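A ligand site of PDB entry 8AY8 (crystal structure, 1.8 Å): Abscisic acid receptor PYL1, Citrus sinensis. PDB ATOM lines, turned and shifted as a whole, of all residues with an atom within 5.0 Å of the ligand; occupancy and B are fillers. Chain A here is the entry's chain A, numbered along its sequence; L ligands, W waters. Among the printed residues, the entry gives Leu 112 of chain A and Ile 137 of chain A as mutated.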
ATOM      1  N   LYS A  88      12.033  12.081   9.570  1.00  0.00           N
ATOM      2  CA  LYS A  88      11.146  11.636  10.634  1.00  0.00           C
ATOM      3  C   LYS A  88       9.702  11.944  10.280  1.00  0.00           C
ATOM      4  O   LYS A  88       9.412  12.897   9.550  1.00  0.00           O
ATOM      5  CB  LYS A  88      11.491  12.301  11.970  1.00  0.00           C
ATOM      6  CG  LYS A  88      12.861  11.933  12.489  1.00  0.00           C
ATOM      7  CD  LYS A  88      13.243  12.753  13.684  1.00  0.00           C
ATOM      8  CE  LYS A  88      13.922  11.863  14.697  1.00  0.00           C
ATOM      9  NZ  LYS A  88      14.728  12.636  15.682  1.00  0.00           N
ATOM     10  N   HIS A  89       8.791  11.127  10.816  1.00  0.00           N
ATOM     11  CA  HIS A  89       7.355  11.296  10.619  1.00  0.00           C
ATOM     12  C   HIS A  89       6.742  12.192  11.698  1.00  0.00           C
ATOM     13  O   HIS A  89       7.376  12.534  12.698  1.00  0.00           O
ATOM     14  CB  HIS A  89       6.654   9.927  10.631  1.00  0.00           C
ATOM     15  CG  HIS A  89       6.929   9.089   9.427  1.00  0.00           C
ATOM     16  ND1 HIS A  89       6.516   9.456   8.160  1.00  0.00           N
ATOM     17  CD2 HIS A  89       7.605   7.924   9.276  1.00  0.00           C
ATOM     18  CE1 HIS A  89       6.899   8.541   7.293  1.00  0.00           C
ATOM     19  NE2 HIS A  89       7.556   7.598   7.946  1.00  0.00           N
ATOM     20  N   PHE A  90       5.482  12.576  11.472  1.00  0.00           N
ATOM     21  CA  PHE A  90       4.570  13.186  12.451  1.00  0.00           C
ATOM     22  C   PHE A  90       4.834  14.664  12.736  1.00  0.00           C
ATOM     23  O   PHE A  90       4.133  15.244  13.578  1.00  0.00           O
ATOM     24  CB  PHE A  90       4.578  12.416  13.781  1.00  0.00           C
ATOM     25  CG  PHE A  90       4.319  10.944  13.623  1.00  0.00           C
ATOM     26  CD1 PHE A  90       3.117  10.488  13.092  1.00  0.00           C
ATOM     27  CD2 PHE A  90       5.285  10.011  13.993  1.00  0.00           C
ATOM     28  CE1 PHE A  90       2.874   9.145  12.939  1.00  0.00           C
ATOM     29  CE2 PHE A  90       5.071   8.659  13.829  1.00  0.00           C
ATOM     30  CZ  PHE A  90       3.843   8.218  13.301  1.00  0.00           C
ATOM     31  N   ILE A  91       5.789  15.301  12.055  1.00  0.00           N
ATOM     32  CA  ILE A  91       6.150  16.684  12.337  1.00  0.00           C
ATOM     33  C   ILE A  91       5.431  17.599  11.356  1.00  0.00           C
ATOM     34  O   ILE A  91       5.551  17.453  10.127  1.00  0.00           O
ATOM     35  CB  ILE A  91       7.667  16.891  12.279  1.00  0.00           C
ATOM     36  CG1 ILE A  91       8.351  16.042  13.342  1.00  0.00           C
ATOM     37  CG2 ILE A  91       8.012  18.366  12.470  1.00  0.00           C
ATOM     38  CD1 ILE A  91       9.889  15.984  13.156  1.00  0.00           C
ATOM     39  N   ARG A 108      14.910  22.813  19.893  1.00  0.00           N
ATOM     40  CA  ARG A 108      13.943  23.016  18.832  1.00  0.00           C
ATOM     41  C   ARG A 108      12.572  22.783  19.429  1.00  0.00           C
ATOM     42  O   ARG A 108      12.401  21.979  20.344  1.00  0.00           O
ATOM     43  CB  ARG A 108      14.194  22.094  17.631  1.00  0.00           C
ATOM     44  CG  ARG A 108      13.856  20.630  17.881  1.00  0.00           C
ATOM     45  CD  ARG A 108      14.392  19.726  16.768  1.00  0.00           C
ATOM     46  NE  ARG A 108      14.241  18.310  17.111  1.00  0.00           N
ATOM     47  CZ  ARG A 108      14.856  17.308  16.495  1.00  0.00           C
ATOM     48  NH1 ARG A 108      15.723  17.519  15.514  1.00  0.00           N
ATOM     49  NH2 ARG A 108      14.598  16.061  16.884  1.00  0.00           N
ATOM     50  N   VAL A 110       8.783  21.674  18.304  1.00  0.00           N
ATOM     51  CA  VAL A 110       8.189  20.907  17.224  1.00  0.00           C
ATOM     52  C   VAL A 110       6.671  20.921  17.408  1.00  0.00           C
ATOM     53  O   VAL A 110       6.192  20.757  18.537  1.00  0.00           O
ATOM     54  CB  VAL A 110       8.736  19.472  17.182  1.00  0.00           C
ATOM     55  CG1 VAL A 110       8.273  18.766  15.931  1.00  0.00           C
ATOM     56  CG2 VAL A 110      10.277  19.472  17.259  1.00  0.00           C
ATOM     57  N   LEU A 112       3.324  18.912  16.106  1.00  0.00           N
ATOM     58  CA  LEU A 112       3.062  17.627  15.470  1.00  0.00           C
ATOM     59  C   LEU A 112       1.798  17.694  14.622  1.00  0.00           C
ATOM     60  O   LEU A 112       0.958  18.563  14.794  1.00  0.00           O
ATOM     61  CB  LEU A 112       2.945  16.543  16.539  1.00  0.00           C
ATOM     62  CG  LEU A 112       4.113  16.442  17.526  1.00  0.00           C
ATOM     63  CD1 LEU A 112       3.841  15.360  18.541  1.00  0.00           C
ATOM     64  CD2 LEU A 112       5.410  16.146  16.779  1.00  0.00           C
ATOM     65  N   LEU A 116      -2.712  12.470  16.922  1.00  0.00           N
ATOM     66  CA  LEU A 116      -1.780  11.666  17.693  1.00  0.00           C
ATOM     67  C   LEU A 116      -1.983  11.860  19.187  1.00  0.00           C
ATOM     68  O   LEU A 116      -2.643  12.817  19.615  1.00  0.00           O
ATOM     69  CB  LEU A 116      -0.334  12.028  17.336  1.00  0.00           C
ATOM     70  CG  LEU A 116      -0.008  12.171  15.854  1.00  0.00           C
ATOM     71  CD1 LEU A 116       1.350  12.848  15.710  1.00  0.00           C
ATOM     72  CD2 LEU A 116      -0.032  10.806  15.171  1.00  0.00           C
ATOM     73  N   PRO A 117      -1.428  10.993  20.000  1.00  0.00           N
ATOM     74  CA  PRO A 117      -1.510  11.183  21.466  1.00  0.00           C
ATOM     75  C   PRO A 117      -0.448  12.158  21.944  1.00  0.00           C
ATOM     76  O   PRO A 117       0.166  11.964  22.994  1.00  0.00           O
ATOM     77  CB  PRO A 117      -1.280   9.771  22.001  1.00  0.00           C
ATOM     78  CG  PRO A 117      -0.368   9.151  20.972  1.00  0.00           C
ATOM     79  CD  PRO A 117      -0.799   9.702  19.649  1.00  0.00           C
ATOM     80  N   ALA A 118      -0.227  13.211  21.156  1.00  0.00           N
ATOM     81  CA  ALA A 118       0.825  14.198  21.371  1.00  0.00           C
ATOM     82  C   ALA A 118       0.524  15.388  20.470  1.00  0.00           C
ATOM     83  O   ALA A 118      -0.066  15.219  19.399  1.00  0.00           O
ATOM     84  CB  ALA A 118       2.214  13.614  21.050  1.00  0.00           C
ATOM     85  N   SER A 121       6.433  19.195  21.043  1.00  0.00           N
ATOM     86  CA  SER A 121       7.643  18.635  21.617  1.00  0.00           C
ATOM     87  C   SER A 121       8.702  19.728  21.667  1.00  0.00           C
ATOM     88  O   SER A 121       8.860  20.462  20.675  1.00  0.00           O
ATOM     89  CB  SER A 121       8.129  17.447  20.790  1.00  0.00           C
ATOM     90  OG  SER A 121       9.198  16.802  21.459  1.00  0.00           O
ATOM     91  N   GLU A 123      12.813  19.937  22.450  1.00  0.00           N
ATOM     92  CA  GLU A 123      13.897  18.960  22.437  1.00  0.00           C
ATOM     93  C   GLU A 123      15.232  19.669  22.445  1.00  0.00           C
ATOM     94  O   GLU A 123      15.379  20.754  21.872  1.00  0.00           O
ATOM     95  CB  GLU A 123      13.783  18.052  21.198  1.00  0.00           C
ATOM     96  CG  GLU A 123      12.313  17.869  20.809  1.00  0.00           C
ATOM     97  CD  GLU A 123      12.095  16.904  19.661  1.00  0.00           C
ATOM     98  OE1 GLU A 123      13.006  16.735  18.828  1.00  0.00           O
ATOM     99  OE2 GLU A 123      11.009  16.296  19.610  1.00  0.00           O
ATOM    100  N   ILE A 137      19.574  13.306  21.766  1.00  0.00           N
ATOM    101  CA  ILE A 137      18.596  14.341  22.051  1.00  0.00           C
ATOM    102  C   ILE A 137      17.836  13.978  23.321  1.00  0.00           C
ATOM    103  O   ILE A 137      17.643  12.802  23.630  1.00  0.00           O
ATOM    104  CB  ILE A 137      17.619  14.532  20.857  1.00  0.00           C
ATOM    105  CG1 ILE A 137      16.852  13.244  20.577  1.00  0.00           C
ATOM    106  CG2 ILE A 137      18.389  14.948  19.607  1.00  0.00           C
ATOM    107  CD1 ILE A 137      15.498  13.117  21.305  1.00  0.00           C
ATOM    108  N   ILE A 139      14.139  15.069  25.368  1.00  0.00           N
ATOM    109  CA  ILE A 139      12.862  15.765  25.284  1.00  0.00           C
ATOM    110  C   ILE A 139      12.659  16.506  26.596  1.00  0.00           C
ATOM    111  O   ILE A 139      12.588  15.891  27.662  1.00  0.00           O
ATOM    112  CB  ILE A 139      11.705  14.785  25.024  1.00  0.00           C
ATOM    113  CG1 ILE A 139      11.904  13.991  23.735  1.00  0.00           C
ATOM    114  CG2 ILE A 139      10.370  15.550  25.003  1.00  0.00           C
ATOM    115  CD1 ILE A 139      12.025  14.832  22.483  1.00  0.00           C
ATOM    116  N   HIS A 144       2.576  15.722  25.503  1.00  0.00           N
ATOM    117  CA  HIS A 144       2.765  14.344  25.045  1.00  0.00           C
ATOM    118  C   HIS A 144       2.984  13.492  26.302  1.00  0.00           C
ATOM    119  O   HIS A 144       3.051  14.013  27.421  1.00  0.00           O
ATOM    120  CB  HIS A 144       3.957  14.205  24.095  1.00  0.00           C
ATOM    121  CG  HIS A 144       5.256  14.683  24.664  1.00  0.00           C
ATOM    122  ND1 HIS A 144       6.021  13.913  25.525  1.00  0.00           N
ATOM    123  CD2 HIS A 144       5.898  15.865  24.547  1.00  0.00           C
ATOM    124  CE1 HIS A 144       7.092  14.599  25.890  1.00  0.00           C
ATOM    125  NE2 HIS A 144       7.043  15.786  25.316  1.00  0.00           N
ATOM    126  N   ARG A 145       3.097  12.175  26.108  1.00  0.00           N
ATOM    127  CA  ARG A 145       3.209  11.243  27.221  1.00  0.00           C
ATOM    128  C   ARG A 145       4.547  10.501  27.249  1.00  0.00           C
ATOM    129  O   ARG A 145       4.647   9.436  27.873  1.00  0.00           O
ATOM    130  CB  ARG A 145       2.051  10.239  27.181  1.00  0.00           C
ATOM    131  CG  ARG A 145       0.699  10.928  26.971  1.00  0.00           C
ATOM    132  CD  ARG A 145      -0.386  10.346  27.866  1.00  0.00           C
ATOM    133  NE  ARG A 145      -0.546   8.926  27.611  1.00  0.00           N
ATOM    134  CZ  ARG A 145      -0.401   7.968  28.514  1.00  0.00           C
ATOM    135  NH1 ARG A 145      -0.240   8.237  29.796  1.00  0.00           N
ATOM    136  NH2 ARG A 145      -0.420   6.702  28.114  1.00  0.00           N
ATOM    137  N   LEU A 146       5.589  11.037  26.622  1.00  0.00           N
ATOM    138  CA  LEU A 146       6.919  10.439  26.685  1.00  0.00           C
ATOM    139  C   LEU A 146       7.835  11.334  27.514  1.00  0.00           C
ATOM    140  O   LEU A 146       8.763  11.973  26.999  1.00  0.00           O
ATOM    141  CB  LEU A 146       7.489  10.208  25.264  1.00  0.00           C
ATOM    142  CG  LEU A 146       6.720   9.189  24.413  1.00  0.00           C
ATOM    143  CD1 LEU A 146       7.423   8.953  23.063  1.00  0.00           C
ATOM    144  CD2 LEU A 146       6.550   7.868  25.148  1.00  0.00           C
ATOM    145  N   TYR A 149      12.059  11.452  27.902  1.00  0.00           N
ATOM    146  CA  TYR A 149      12.593  10.687  26.796  1.00  0.00           C
ATOM    147  C   TYR A 149      13.995  11.172  26.457  1.00  0.00           C
ATOM    148  O   TYR A 149      14.224  12.381  26.321  1.00  0.00           O
ATOM    149  CB  TYR A 149      11.679  10.827  25.595  1.00  0.00           C
ATOM    150  CG  TYR A 149      11.962   9.920  24.404  1.00  0.00           C
ATOM    151  CD1 TYR A 149      12.820  10.327  23.379  1.00  0.00           C
ATOM    152  CD2 TYR A 149      11.321   8.704  24.280  1.00  0.00           C
ATOM    153  CE1 TYR A 149      13.041   9.518  22.273  1.00  0.00           C
ATOM    154  CE2 TYR A 149      11.539   7.888  23.181  1.00  0.00           C
ATOM    155  CZ  TYR A 149      12.400   8.295  22.184  1.00  0.00           C
ATOM    156  OH  TYR A 149      12.594   7.477  21.088  1.00  0.00           O
ATOM    157  N   PHE A 188       4.618   1.243  21.856  1.00  0.00           N
ATOM    158  CA  PHE A 188       4.384   2.555  21.266  1.00  0.00           C
ATOM    159  C   PHE A 188       5.697   3.194  20.794  1.00  0.00           C
ATOM    160  O   PHE A 188       5.856   3.517  19.613  1.00  0.00           O
ATOM    161  CB  PHE A 188       3.660   3.451  22.279  1.00  0.00           C
ATOM    162  CG  PHE A 188       3.494   4.875  21.844  1.00  0.00           C
ATOM    163  CD1 PHE A 188       2.597   5.213  20.838  1.00  0.00           C
ATOM    164  CD2 PHE A 188       4.214   5.889  22.473  1.00  0.00           C
ATOM    165  CE1 PHE A 188       2.409   6.548  20.456  1.00  0.00           C
ATOM    166  CE2 PHE A 188       4.048   7.220  22.096  1.00  0.00           C
ATOM    167  CZ  PHE A 188       3.135   7.551  21.092  1.00  0.00           C
ATOM    168  N   VAL A 192       7.162   3.999  16.773  1.00  0.00           N
ATOM    169  CA  VAL A 192       7.564   5.286  16.226  1.00  0.00           C
ATOM    170  C   VAL A 192       9.019   5.254  15.765  1.00  0.00           C
ATOM    171  O   VAL A 192       9.348   5.774  14.699  1.00  0.00           O
ATOM    172  CB  VAL A 192       7.301   6.404  17.249  1.00  0.00           C
ATOM    173  CG1 VAL A 192       7.878   7.726  16.754  1.00  0.00           C
ATOM    174  CG2 VAL A 192       5.797   6.553  17.495  1.00  0.00           C
ATOM    175  N   ASN A 196      10.309   5.757  11.810  1.00  0.00           N
ATOM    176  CA  ASN A 196      11.278   6.789  11.443  1.00  0.00           C
ATOM    177  C   ASN A 196      12.531   6.185  10.818  1.00  0.00           C
ATOM    178  O   ASN A 196      13.092   6.764   9.882  1.00  0.00           O
ATOM    179  CB  ASN A 196      11.635   7.618  12.677  1.00  0.00           C
ATOM    180  CG  ASN A 196      10.521   8.573  13.064  1.00  0.00           C
ATOM    181  OD1 ASN A 196       9.651   8.862  12.255  1.00  0.00           O
ATOM    182  ND2 ASN A 196      10.541   9.071  14.295  1.00  0.00           N
HETATM  183  C1  LIG L   1       8.034  13.945  17.878  1.00  0.00           C
HETATM  184  N1  LIG L   1       5.119  11.531  19.733  1.00  0.00           N
HETATM  185  C2  LIG L   1       6.211  12.378  17.718  1.00  0.00           C
HETATM  186  C3  LIG L   1       6.118  12.318  19.109  1.00  0.00           C
HETATM  187  C4  LIG L   1       7.007  13.070  19.893  1.00  0.00           C
HETATM  188  C5  LIG L   1       7.949  13.880  19.254  1.00  0.00           C
HETATM  189  C6  LIG L   1       6.913  12.957  21.335  1.00  0.00           C
HETATM  190  C7  LIG L   1       4.012  10.965  18.944  1.00  0.00           C
HETATM  191  C8  LIG L   1       9.008  14.897  17.220  1.00  0.00           C
HETATM  192  C9  LIG L   1       9.599  10.158  19.166  1.00  0.00           C
HETATM  193  C10 LIG L   1       7.885  13.695  22.216  1.00  0.00           C
HETATM  194  C11 LIG L   1      10.749  12.168  18.564  1.00  0.00           C
HETATM  195  C12 LIG L   1       9.981  11.078  18.204  1.00  0.00           C
HETATM  196  C13 LIG L   1       9.987  10.328  20.487  1.00  0.00           C
HETATM  197  C14 LIG L   1      10.762  11.413  20.832  1.00  0.00           C
HETATM  198  C15 LIG L   1      11.152  12.345  19.884  1.00  0.00           C
HETATM  199  C16 LIG L   1       4.390   9.688  18.315  1.00  0.00           C
HETATM  200  C17 LIG L   1       7.162  13.177  17.114  1.00  0.00           C
HETATM  201  C18 LIG L   1       5.972  12.148  21.867  1.00  0.00           C
HETATM  202  C19 LIG L   1       5.029  11.396  21.118  1.00  0.00           C
HETATM  203  N2  LIG L   1      10.386  14.733  17.708  1.00  0.00           N
HETATM  204  O1  LIG L   1      12.580  13.652  17.507  1.00  0.00           O
HETATM  205  O2  LIG L   1      10.690  12.918  16.103  1.00  0.00           O
HETATM  206  O3  LIG L   1       4.151  10.686  21.606  1.00  0.00           O
HETATM  207  S1  LIG L   1      11.184  13.373  17.360  1.00  0.00           S
HETATM  208  O   HOH W   1       8.765  11.367  14.688  1.00  0.00           O
HETATM  209  O   HOH W   2       2.442  10.384  23.714  1.00  0.00           O
HETATM  210  O   HOH W   3       9.932   6.946  19.697  1.00  0.00           O
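Water W2 lies within hydrogen-bond range of an oxygen (O3) of the ligand, the backbone carbonyl oxygen (O) of Pro 117 and the backbone NH (N) of Arg 145. Water W1 lies within hydrogen-bond range of O of His 89 (2.7 Å), O2 of the ligand (2.8 Å) and ND2 of Asn 196 (2.9 Å).
A nitrogen (N2) of the ligand is in hydrogen-bond range of the side-chain carboxylate (OE2) of Glu 123 (2.5 Å). O1 of the ligand sits at hydrogen-bond distance from NH2 of Arg 108 (3.2 Å). The side-chain amino group (NZ) of Lys 88 lies within hydrogen-bond range of an oxygen (O1) of the ligand.
CD2 of Leu 112 touches C17 of the ligand (3.5 Å). CB of Ala 118 touches O3 of the ligand, 3.6 Å away. Ser 121 touches the ligand (OG to C10, 3.5 Å). CD1 of Ile 139 touches C15 of the ligand (3.7 Å). His 144 touches the ligand (CB to C18, 3.6 Å). Leu 146 touches the ligand. Tyr 149 touches the ligand (CE1 to C14, 3.3 Å). CZ of Phe 188 touches O3 of the ligand, at 3.3 Å. Val 192 touches the ligand (CG2 to C16, 3.5 Å). 12 residues have an atom within 4 Å of the ligand: Lys 88, Arg 108, Leu 112, Ala 118, Ser 121, Glu 123, Ile 139, His 144, Leu 146, Tyr 149, Phe 188 and Val 192.
The side-chain carboxylate (OE2) of Glu 123 lies within hydrogen-bond range of the side-chain hydroxyl (OG) of Ser 121 (2.6 Å). The backbone NH (N) of Val 110 is in hydrogen-bond range of the backbone carbonyl oxygen (O) of Ser 121, 2.7 Å away. The side-chain carboxylate (OE1) of Glu 123 lies within salt-bridge range of the guanidinium group (NH2) of Arg 108. O of Tyr 149 is in hydrogen-bond range of N of Ile 139 (2.9 Å). A ring nitrogen (ND1) of His 144 lies within hydrogen-bond range of the backbone NH (N) of Leu 146.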
